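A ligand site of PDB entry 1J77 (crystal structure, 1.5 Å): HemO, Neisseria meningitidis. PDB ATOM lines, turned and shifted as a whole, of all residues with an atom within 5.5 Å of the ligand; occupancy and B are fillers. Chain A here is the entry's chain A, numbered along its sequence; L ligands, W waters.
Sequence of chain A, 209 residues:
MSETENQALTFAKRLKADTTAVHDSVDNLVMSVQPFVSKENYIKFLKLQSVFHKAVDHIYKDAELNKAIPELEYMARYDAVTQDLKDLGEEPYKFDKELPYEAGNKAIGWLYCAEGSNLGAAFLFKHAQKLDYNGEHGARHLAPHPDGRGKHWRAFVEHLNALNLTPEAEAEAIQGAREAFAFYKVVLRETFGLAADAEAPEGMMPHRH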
ATOM      1  N   ALA A  12       2.919 -39.151   8.354  1.00  0.00           N
ATOM      2  CA  ALA A  12       2.902 -37.902   9.080  1.00  0.00           C
ATOM      3  C   ALA A  12       4.154 -37.113   8.789  1.00  0.00           C
ATOM      4  O   ALA A  12       4.104 -35.882   8.722  1.00  0.00           O
ATOM      5  CB  ALA A  12       2.735 -38.175  10.587  1.00  0.00           C
ATOM      6  N   LYS A  16       4.444 -33.405   6.789  1.00  0.00           N
ATOM      7  CA  LYS A  16       5.260 -32.292   7.319  1.00  0.00           C
ATOM      8  C   LYS A  16       6.293 -31.831   6.306  1.00  0.00           C
ATOM      9  O   LYS A  16       6.413 -30.631   6.030  1.00  0.00           O
ATOM     10  CB  LYS A  16       6.006 -32.709   8.600  1.00  0.00           C
ATOM     11  CG  LYS A  16       6.795 -31.570   9.274  1.00  0.00           C
ATOM     12  CD  LYS A  16       7.413 -32.037  10.585  1.00  0.00           C
ATOM     13  CE  LYS A  16       8.459 -31.083  11.115  1.00  0.00           C
ATOM     14  NZ  LYS A  16       7.838 -29.847  11.655  1.00  0.00           N
ATOM     15  N   HIS A  23       3.609 -23.870   5.226  1.00  0.00           N
ATOM     16  CA  HIS A  23       3.299 -23.571   6.607  1.00  0.00           C
ATOM     17  C   HIS A  23       4.016 -22.269   7.053  1.00  0.00           C
ATOM     18  O   HIS A  23       3.438 -21.393   7.637  1.00  0.00           O
ATOM     19  CB  HIS A  23       3.778 -24.695   7.587  1.00  0.00           C
ATOM     20  CG  HIS A  23       3.619 -24.307   9.024  1.00  0.00           C
ATOM     21  ND1 HIS A  23       4.551 -23.544   9.702  1.00  0.00           N
ATOM     22  CD2 HIS A  23       2.570 -24.458   9.858  1.00  0.00           C
ATOM     23  CE1 HIS A  23       4.080 -23.281  10.913  1.00  0.00           C
ATOM     24  NE2 HIS A  23       2.895 -23.865  11.042  1.00  0.00           N
ATOM     25  N   VAL A  26       2.445 -19.205   5.902  1.00  0.00           N
ATOM     26  CA  VAL A  26       1.265 -18.871   6.687  1.00  0.00           C
ATOM     27  C   VAL A  26       1.619 -18.161   7.992  1.00  0.00           C
ATOM     28  O   VAL A  26       1.074 -17.101   8.310  1.00  0.00           O
ATOM     29  CB  VAL A  26       0.406 -20.164   6.946  1.00  0.00           C
ATOM     30  CG1 VAL A  26      -0.658 -19.856   7.995  1.00  0.00           C
ATOM     31  CG2 VAL A  26      -0.203 -20.618   5.649  1.00  0.00           C
ATOM     32  N   ASP A  27       2.605 -18.711   8.703  1.00  0.00           N
ATOM     33  CA  ASP A  27       3.119 -18.146   9.938  1.00  0.00           C
ATOM     34  C   ASP A  27       3.555 -16.685   9.666  1.00  0.00           C
ATOM     35  O   ASP A  27       3.096 -15.767  10.306  1.00  0.00           O
ATOM     36  CB  ASP A  27       4.280 -19.057  10.404  1.00  0.00           C
ATOM     37  CG  ASP A  27       5.076 -18.536  11.635  1.00  0.00           C
ATOM     38  OD1 ASP A  27       4.949 -17.365  12.059  1.00  0.00           O
ATOM     39  OD2 ASP A  27       5.796 -19.364  12.273  1.00  0.00           O
ATOM     40  N   ASN A  28       4.368 -16.506   8.629  1.00  0.00           N
ATOM     41  CA  ASN A  28       4.849 -15.168   8.296  1.00  0.00           C
ATOM     42  C   ASN A  28       3.731 -14.219   7.926  1.00  0.00           C
ATOM     43  O   ASN A  28       3.747 -13.037   8.326  1.00  0.00           O
ATOM     44  CB  ASN A  28       5.833 -15.268   7.106  1.00  0.00           C
ATOM     45  CG  ASN A  28       7.163 -15.862   7.483  1.00  0.00           C
ATOM     46  OD1 ASN A  28       7.565 -15.787   8.633  1.00  0.00           O
ATOM     47  ND2 ASN A  28       7.868 -16.448   6.506  1.00  0.00           N
ATOM     48  N   VAL A  30       0.455 -14.378   8.763  1.00  0.00           N
ATOM     49  CA  VAL A  30      -0.351 -14.080   9.944  1.00  0.00           C
ATOM     50  C   VAL A  30       0.381 -13.002  10.775  1.00  0.00           C
ATOM     51  O   VAL A  30      -0.197 -11.986  11.165  1.00  0.00           O
ATOM     52  CB  VAL A  30      -0.562 -15.331  10.809  1.00  0.00           C
ATOM     53  CG1 VAL A  30      -1.041 -14.961  12.252  1.00  0.00           C
ATOM     54  CG2 VAL A  30      -1.510 -16.346  10.091  1.00  0.00           C
ATOM     55  N   MET A  31       1.644 -13.222  11.038  1.00  0.00           N
ATOM     56  CA  MET A  31       2.332 -12.203  11.840  1.00  0.00           C
ATOM     57  C   MET A  31       2.465 -10.855  11.148  1.00  0.00           C
ATOM     58  O   MET A  31       2.318  -9.829  11.807  1.00  0.00           O
ATOM     59  CB  MET A  31       3.651 -12.735  12.303  1.00  0.00           C
ATOM     60  CG  MET A  31       3.555 -13.976  13.169  1.00  0.00           C
ATOM     61  SD  MET A  31       2.482 -13.764  14.622  1.00  0.00           S
ATOM     62  CE  MET A  31       3.376 -12.524  15.503  1.00  0.00           C
ATOM     63  N   GLN A  49      -9.982 -17.355  11.770  1.00  0.00           N
ATOM     64  CA  GLN A  49      -9.969 -18.621  12.467  1.00  0.00           C
ATOM     65  C   GLN A  49     -11.357 -19.277  12.387  1.00  0.00           C
ATOM     66  O   GLN A  49     -11.469 -20.500  12.222  1.00  0.00           O
ATOM     67  CB  GLN A  49      -9.529 -18.449  13.935  1.00  0.00           C
ATOM     68  CG  GLN A  49      -8.099 -17.962  14.154  1.00  0.00           C
ATOM     69  CD  GLN A  49      -7.108 -19.084  14.029  1.00  0.00           C
ATOM     70  OE1 GLN A  49      -6.603 -19.613  15.035  1.00  0.00           O
ATOM     71  NE2 GLN A  49      -6.793 -19.465  12.779  1.00  0.00           N
ATOM     72  N   PHE A  52     -11.920 -20.908   8.874  1.00  0.00           N
ATOM     73  CA  PHE A  52     -11.126 -22.114   8.715  1.00  0.00           C
ATOM     74  C   PHE A  52     -11.689 -23.278   9.527  1.00  0.00           C
ATOM     75  O   PHE A  52     -11.796 -24.422   9.052  1.00  0.00           O
ATOM     76  CB  PHE A  52      -9.646 -21.884   9.062  1.00  0.00           C
ATOM     77  CG  PHE A  52      -8.811 -23.117   8.862  1.00  0.00           C
ATOM     78  CD1 PHE A  52      -8.453 -23.534   7.593  1.00  0.00           C
ATOM     79  CD2 PHE A  52      -8.410 -23.854   9.925  1.00  0.00           C
ATOM     80  CE1 PHE A  52      -7.694 -24.701   7.418  1.00  0.00           C
ATOM     81  CE2 PHE A  52      -7.650 -25.007   9.720  1.00  0.00           C
ATOM     82  CZ  PHE A  52      -7.317 -25.387   8.494  1.00  0.00           C
ATOM     83  N   TYR A 112      -5.180 -32.983   9.040  1.00  0.00           N
ATOM     84  CA  TYR A 112      -3.771 -32.788   9.445  1.00  0.00           C
ATOM     85  C   TYR A 112      -3.479 -31.288   9.665  1.00  0.00           C
ATOM     86  O   TYR A 112      -2.987 -30.892  10.742  1.00  0.00           O
ATOM     87  CB  TYR A 112      -2.846 -33.392   8.379  1.00  0.00           C
ATOM     88  CG  TYR A 112      -1.419 -32.898   8.518  1.00  0.00           C
ATOM     89  CD1 TYR A 112      -0.561 -33.417   9.502  1.00  0.00           C
ATOM     90  CD2 TYR A 112      -0.950 -31.902   7.689  1.00  0.00           C
ATOM     91  CE1 TYR A 112       0.728 -32.931   9.643  1.00  0.00           C
ATOM     92  CE2 TYR A 112       0.331 -31.381   7.840  1.00  0.00           C
ATOM     93  CZ  TYR A 112       1.178 -31.903   8.815  1.00  0.00           C
ATOM     94  OH  TYR A 112       2.487 -31.380   8.941  1.00  0.00           O
ATOM     95  N   CYS A 113      -3.880 -30.446   8.727  1.00  0.00           N
ATOM     96  CA  CYS A 113      -3.601 -28.993   8.791  1.00  0.00           C
ATOM     97  C   CYS A 113      -4.284 -28.408  10.002  1.00  0.00           C
ATOM     98  O   CYS A 113      -3.672 -27.712  10.799  1.00  0.00           O
ATOM     99  CB  CYS A 113      -4.110 -28.387   7.525  1.00  0.00           C
ATOM    100  SG  CYS A 113      -3.802 -26.678   7.336  1.00  0.00           S
ATOM    101  N   ALA A 114      -5.588 -28.688  10.181  1.00  0.00           N
ATOM    102  CA  ALA A 114      -6.249 -28.131  11.327  1.00  0.00           C
ATOM    103  C   ALA A 114      -5.730 -28.637  12.663  1.00  0.00           C
ATOM    104  O   ALA A 114      -5.647 -27.880  13.636  1.00  0.00           O
ATOM    105  CB  ALA A 114      -7.808 -28.353  11.233  1.00  0.00           C
ATOM    106  N   GLU A 115      -5.436 -29.940  12.737  1.00  0.00           N
ATOM    107  CA  GLU A 115      -5.039 -30.479  13.994  1.00  0.00           C
ATOM    108  C   GLU A 115      -3.608 -30.033  14.347  1.00  0.00           C
ATOM    109  O   GLU A 115      -3.322 -29.710  15.518  1.00  0.00           O
ATOM    110  CB  GLU A 115      -5.278 -31.993  14.042  1.00  0.00           C
ATOM    111  CG  GLU A 115      -5.213 -32.553  15.476  1.00  0.00           C
ATOM    112  CD  GLU A 115      -6.139 -31.891  16.450  1.00  0.00           C
ATOM    113  OE1 GLU A 115      -7.310 -31.615  16.130  1.00  0.00           O
ATOM    114  OE2 GLU A 115      -5.713 -31.664  17.594  1.00  0.00           O
ATOM    115  N   GLY A 116      -2.738 -29.980  13.353  1.00  0.00           N
ATOM    116  CA  GLY A 116      -1.419 -29.441  13.580  1.00  0.00           C
ATOM    117  C   GLY A 116      -1.409 -27.983  14.014  1.00  0.00           C
ATOM    118  O   GLY A 116      -0.519 -27.586  14.754  1.00  0.00           O
ATOM    119  N   SER A 117      -2.397 -27.202  13.623  1.00  0.00           N
ATOM    120  CA  SER A 117      -2.467 -25.818  14.011  1.00  0.00           C
ATOM    121  C   SER A 117      -2.621 -25.638  15.521  1.00  0.00           C
ATOM    122  O   SER A 117      -2.225 -24.607  16.079  1.00  0.00           O
ATOM    123  CB  SER A 117      -3.593 -25.129  13.250  1.00  0.00           C
ATOM    124  OG  SER A 117      -4.890 -25.349  13.826  1.00  0.00           O
ATOM    125  N   LEU A 119      -1.357 -27.886  17.675  1.00  0.00           N
ATOM    126  CA  LEU A 119      -0.004 -28.256  18.104  1.00  0.00           C
ATOM    127  C   LEU A 119       0.804 -26.977  18.249  1.00  0.00           C
ATOM    128  O   LEU A 119       1.340 -26.663  19.313  1.00  0.00           O
ATOM    129  CB  LEU A 119       0.660 -29.144  17.045  1.00  0.00           C
ATOM    130  CG  LEU A 119       1.816 -30.031  17.472  1.00  0.00           C
ATOM    131  CD1 LEU A 119       2.874 -30.143  16.394  1.00  0.00           C
ATOM    132  CD2 LEU A 119       2.377 -29.639  18.819  1.00  0.00           C
ATOM    133  N   GLY A 120       0.831 -26.202  17.186  1.00  0.00           N
ATOM    134  CA  GLY A 120       1.652 -25.022  17.150  1.00  0.00           C
ATOM    135  C   GLY A 120       1.073 -23.722  17.624  1.00  0.00           C
ATOM    136  O   GLY A 120       1.712 -22.699  17.420  1.00  0.00           O
ATOM    137  N   PHE A 123       2.567 -20.198  20.560  1.00  0.00           N
ATOM    138  CA  PHE A 123       3.109 -18.844  20.357  1.00  0.00           C
ATOM    139  C   PHE A 123       1.959 -17.883  20.296  1.00  0.00           C
ATOM    140  O   PHE A 123       1.968 -16.820  20.917  1.00  0.00           O
ATOM    141  CB  PHE A 123       3.958 -18.807  19.089  1.00  0.00           C
ATOM    142  CG  PHE A 123       4.476 -17.463  18.754  1.00  0.00           C
ATOM    143  CD1 PHE A 123       5.721 -17.061  19.221  1.00  0.00           C
ATOM    144  CD2 PHE A 123       3.751 -16.626  17.928  1.00  0.00           C
ATOM    145  CE1 PHE A 123       6.227 -15.812  18.902  1.00  0.00           C
ATOM    146  CE2 PHE A 123       4.247 -15.371  17.621  1.00  0.00           C
ATOM    147  CZ  PHE A 123       5.490 -14.967  18.102  1.00  0.00           C
ATOM    148  N   LEU A 124       0.927 -18.208  19.535  1.00  0.00           N
ATOM    149  CA  LEU A 124      -0.210 -17.340  19.422  1.00  0.00           C
ATOM    150  C   LEU A 124      -0.903 -17.164  20.776  1.00  0.00           C
ATOM    151  O   LEU A 124      -1.406 -16.069  21.075  1.00  0.00           O
ATOM    152  CB  LEU A 124      -1.203 -17.865  18.401  1.00  0.00           C
ATOM    153  CG  LEU A 124      -0.771 -17.873  16.941  1.00  0.00           C
ATOM    154  CD1 LEU A 124      -1.783 -18.664  16.211  1.00  0.00           C
ATOM    155  CD2 LEU A 124      -0.657 -16.449  16.353  1.00  0.00           C
ATOM    156  N   TRP A 153      -0.841 -34.439  20.225  1.00  0.00           N
ATOM    157  CA  TRP A 153      -0.399 -34.540  18.848  1.00  0.00           C
ATOM    158  C   TRP A 153       0.236 -35.898  18.525  1.00  0.00           C
ATOM    159  O   TRP A 153      -0.074 -36.492  17.487  1.00  0.00           O
ATOM    160  CB  TRP A 153       0.585 -33.368  18.520  1.00  0.00           C
ATOM    161  CG  TRP A 153       1.205 -33.440  17.209  1.00  0.00           C
ATOM    162  CD1 TRP A 153       2.485 -33.705  16.934  1.00  0.00           C
ATOM    163  CD2 TRP A 153       0.558 -33.191  15.947  1.00  0.00           C
ATOM    164  NE1 TRP A 153       2.698 -33.710  15.579  1.00  0.00           N
ATOM    165  CE2 TRP A 153       1.523 -33.383  14.936  1.00  0.00           C
ATOM    166  CE3 TRP A 153      -0.765 -32.910  15.561  1.00  0.00           C
ATOM    167  CZ2 TRP A 153       1.236 -33.277  13.604  1.00  0.00           C
ATOM    168  CZ3 TRP A 153      -1.042 -32.777  14.242  1.00  0.00           C
ATOM    169  CH2 TRP A 153      -0.071 -32.963  13.267  1.00  0.00           C
ATOM    170  N   ALA A 180      -5.532 -26.846   2.004  1.00  0.00           N
ATOM    171  CA  ALA A 180      -6.020 -26.283   3.303  1.00  0.00           C
ATOM    172  C   ALA A 180      -5.200 -25.054   3.678  1.00  0.00           C
ATOM    173  O   ALA A 180      -5.769 -24.021   4.002  1.00  0.00           O
ATOM    174  CB  ALA A 180      -5.950 -27.274   4.346  1.00  0.00           C
ATOM    175  N   PHE A 181      -3.882 -25.176   3.536  1.00  0.00           N
ATOM    176  CA  PHE A 181      -3.024 -24.008   3.801  1.00  0.00           C
ATOM    177  C   PHE A 181      -3.311 -22.900   2.829  1.00  0.00           C
ATOM    178  O   PHE A 181      -3.321 -21.730   3.220  1.00  0.00           O
ATOM    179  CB  PHE A 181      -1.537 -24.357   3.751  1.00  0.00           C
ATOM    180  CG  PHE A 181      -0.972 -25.051   4.992  1.00  0.00           C
ATOM    181  CD1 PHE A 181      -0.404 -26.338   4.895  1.00  0.00           C
ATOM    182  CD2 PHE A 181      -0.961 -24.437   6.243  1.00  0.00           C
ATOM    183  CE1 PHE A 181       0.148 -26.947   5.989  1.00  0.00           C
ATOM    184  CE2 PHE A 181      -0.380 -25.060   7.327  1.00  0.00           C
ATOM    185  CZ  PHE A 181       0.151 -26.346   7.196  1.00  0.00           C
ATOM    186  N   TYR A 184      -6.501 -21.141   3.840  1.00  0.00           N
ATOM    187  CA  TYR A 184      -6.246 -20.277   4.978  1.00  0.00           C
ATOM    188  C   TYR A 184      -5.746 -18.913   4.552  1.00  0.00           C
ATOM    189  O   TYR A 184      -6.252 -17.894   5.038  1.00  0.00           O
ATOM    190  CB  TYR A 184      -5.294 -20.908   5.966  1.00  0.00           C
ATOM    191  CG  TYR A 184      -5.246 -20.213   7.328  1.00  0.00           C
ATOM    192  CD1 TYR A 184      -6.084 -20.552   8.364  1.00  0.00           C
ATOM    193  CD2 TYR A 184      -4.369 -19.186   7.574  1.00  0.00           C
ATOM    194  CE1 TYR A 184      -6.043 -19.906   9.587  1.00  0.00           C
ATOM    195  CE2 TYR A 184      -4.328 -18.541   8.797  1.00  0.00           C
ATOM    196  CZ  TYR A 184      -5.112 -18.920   9.802  1.00  0.00           C
ATOM    197  OH  TYR A 184      -5.092 -18.259  10.999  1.00  0.00           O
HETATM  198  C1  LIG L   1       3.273 -26.871  13.681  1.00  0.00           C
HETATM  199  C2  LIG L   1       4.080 -22.187  14.611  1.00  0.00           C
HETATM  200  C3  LIG L   1      -0.029 -21.029  12.242  1.00  0.00           C
HETATM  201  C4  LIG L   1      -0.551 -25.696  10.912  1.00  0.00           C
HETATM  202  C5  LIG L   1       3.794 -25.717  14.222  1.00  0.00           C
HETATM  203  C6  LIG L   1       4.902 -25.627  15.198  1.00  0.00           C
HETATM  204  C7  LIG L   1       5.092 -24.329  15.425  1.00  0.00           C
HETATM  205  C8  LIG L   1       4.162 -23.544  14.624  1.00  0.00           C
HETATM  206  C9  LIG L   1       6.152 -23.728  16.390  1.00  0.00           C
HETATM  207  C10 LIG L   1       5.679 -26.773  15.907  1.00  0.00           C
HETATM  208  C11 LIG L   1       5.027 -27.028  17.263  1.00  0.00           C
HETATM  209  C12 LIG L   1       5.632 -28.236  17.968  1.00  0.00           C
HETATM  210  O1  LIG L   1       6.273 -29.068  17.273  1.00  0.00           O
HETATM  211  O2  LIG L   1       5.478 -28.316  19.218  1.00  0.00           O
HETATM  212  C13 LIG L   1       3.036 -21.449  14.058  1.00  0.00           C
HETATM  213  C14 LIG L   1       2.878 -20.029  14.178  1.00  0.00           C
HETATM  214  C15 LIG L   1       1.751 -19.687  13.490  1.00  0.00           C
HETATM  215  C16 LIG L   1       1.153 -20.920  12.997  1.00  0.00           C
HETATM  216  C17 LIG L   1       3.883 -19.154  14.970  1.00  0.00           C
HETATM  217  C18 LIG L   1       1.104 -18.304  13.357  1.00  0.00           C
HETATM  218  C19 LIG L   1       1.841 -17.204  13.281  1.00  0.00           C
HETATM  219  C20 LIG L   1      -0.542 -22.201  11.733  1.00  0.00           C
HETATM  220  C21 LIG L   1      -1.813 -22.338  11.032  1.00  0.00           C
HETATM  221  C22 LIG L   1      -1.910 -23.609  10.615  1.00  0.00           C
HETATM  222  C23 LIG L   1      -0.798 -24.363  11.122  1.00  0.00           C
HETATM  223  C24 LIG L   1      -2.750 -21.157  10.720  1.00  0.00           C
HETATM  224  C25 LIG L   1      -3.038 -24.265   9.818  1.00  0.00           C
HETATM  225  C26 LIG L   1      -3.865 -23.508   9.108  1.00  0.00           C
HETATM  226  C27 LIG L   1       0.446 -26.386  11.532  1.00  0.00           C
HETATM  227  C28 LIG L   1       0.609 -27.810  11.370  1.00  0.00           C
HETATM  228  C29 LIG L   1       1.797 -28.183  12.192  1.00  0.00           C
HETATM  229  C30 LIG L   1       2.220 -26.943  12.803  1.00  0.00           C
HETATM  230  C31 LIG L   1      -0.267 -28.708  10.492  1.00  0.00           C
HETATM  231  C32 LIG L   1       2.386 -29.573  12.440  1.00  0.00           C
HETATM  232  C33 LIG L   1       3.720 -29.763  11.770  1.00  0.00           C
HETATM  233  C34 LIG L   1       4.068 -31.215  12.032  1.00  0.00           C
HETATM  234  O3  LIG L   1       3.639 -32.071  11.236  1.00  0.00           O
HETATM  235  O4  LIG L   1       4.835 -31.491  13.006  1.00  0.00           O
HETATM  236  N1  LIG L   1       3.375 -24.444  13.917  1.00  0.00           N
HETATM  237  N2  LIG L   1       1.999 -21.959  13.302  1.00  0.00           N
HETATM  238  N3  LIG L   1       0.009 -23.443  11.772  1.00  0.00           N
HETATM  239  N4  LIG L   1       1.419 -25.874  12.394  1.00  0.00           N
HETATM  240 FE1  LIG L   1       1.770 -23.928  12.761  1.00  0.00          FE
HETATM  241  O   HOH W   1       6.184 -16.672  14.354  1.00  0.00           O
HETATM  242  O   HOH W   2       3.690 -26.834  20.799  1.00  0.00           O
HETATM  243  O   HOH W   3       6.451 -29.902  14.471  1.00  0.00           O
HETATM  244  O   HOH W   4       6.492 -20.615  17.615  1.00  0.00           O
HETATM  245  O   HOH W   5       0.622 -24.191  14.312  1.00  0.00           O
HETATM  246  O   HOH W   6      -1.509 -22.198  15.099  1.00  0.00           O
HETATM  247  O   HOH W   7       4.196 -34.700  11.446  1.00  0.00           O
HETATM  248  O   HOH W   8       5.246 -33.398  14.785  1.00  0.00           O
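NE2 of His 23 is bound to FE1 of the ligand, 2.1 Å away.
The side-chain amino group of Lys 16 is in salt-bridge range of an oxygen (O4) of the ligand, 3.7 Å away.
OH of Tyr 112 sits at hydrogen-bond distance from O3 of the ligand (2.7 Å).
The side-chain amide nitrogen (NE2) of Gln 49 is in hydrogen-bond range of the side-chain hydroxyl (OH) of Tyr 184, at 2.7 Å.
The side-chain hydroxyl of Ser 117 sits at hydrogen-bond distance from the backbone carbonyl oxygen of Ala 114 (2.6 Å).
Residues that only touch the ligand: Val 26, Asp 27, Val 30, Met 31, Phe 52, Cys 113, Gly 116, Ser 117, Leu 119, Gly 120, Phe 123, Leu 124, Trp 153, Phe 181 and Tyr 184.
Along chain A the residues within 4 Å of the ligand span positions 16 to 184.
Water W8 lies within hydrogen-bond range of O4 of the ligand and NE1 of Trp 153.
Water W7 bridges O3 of the ligand and O of Ala 12.
Water W3 bridges an oxygen (O4) of the ligand (2.7 Å) and the side-chain amino group (NZ) of Lys 16 (3.1 Å).
Water W2 bridges O of Leu 119 (2.8 Å) and O2 of the ligand (2.8 Å).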
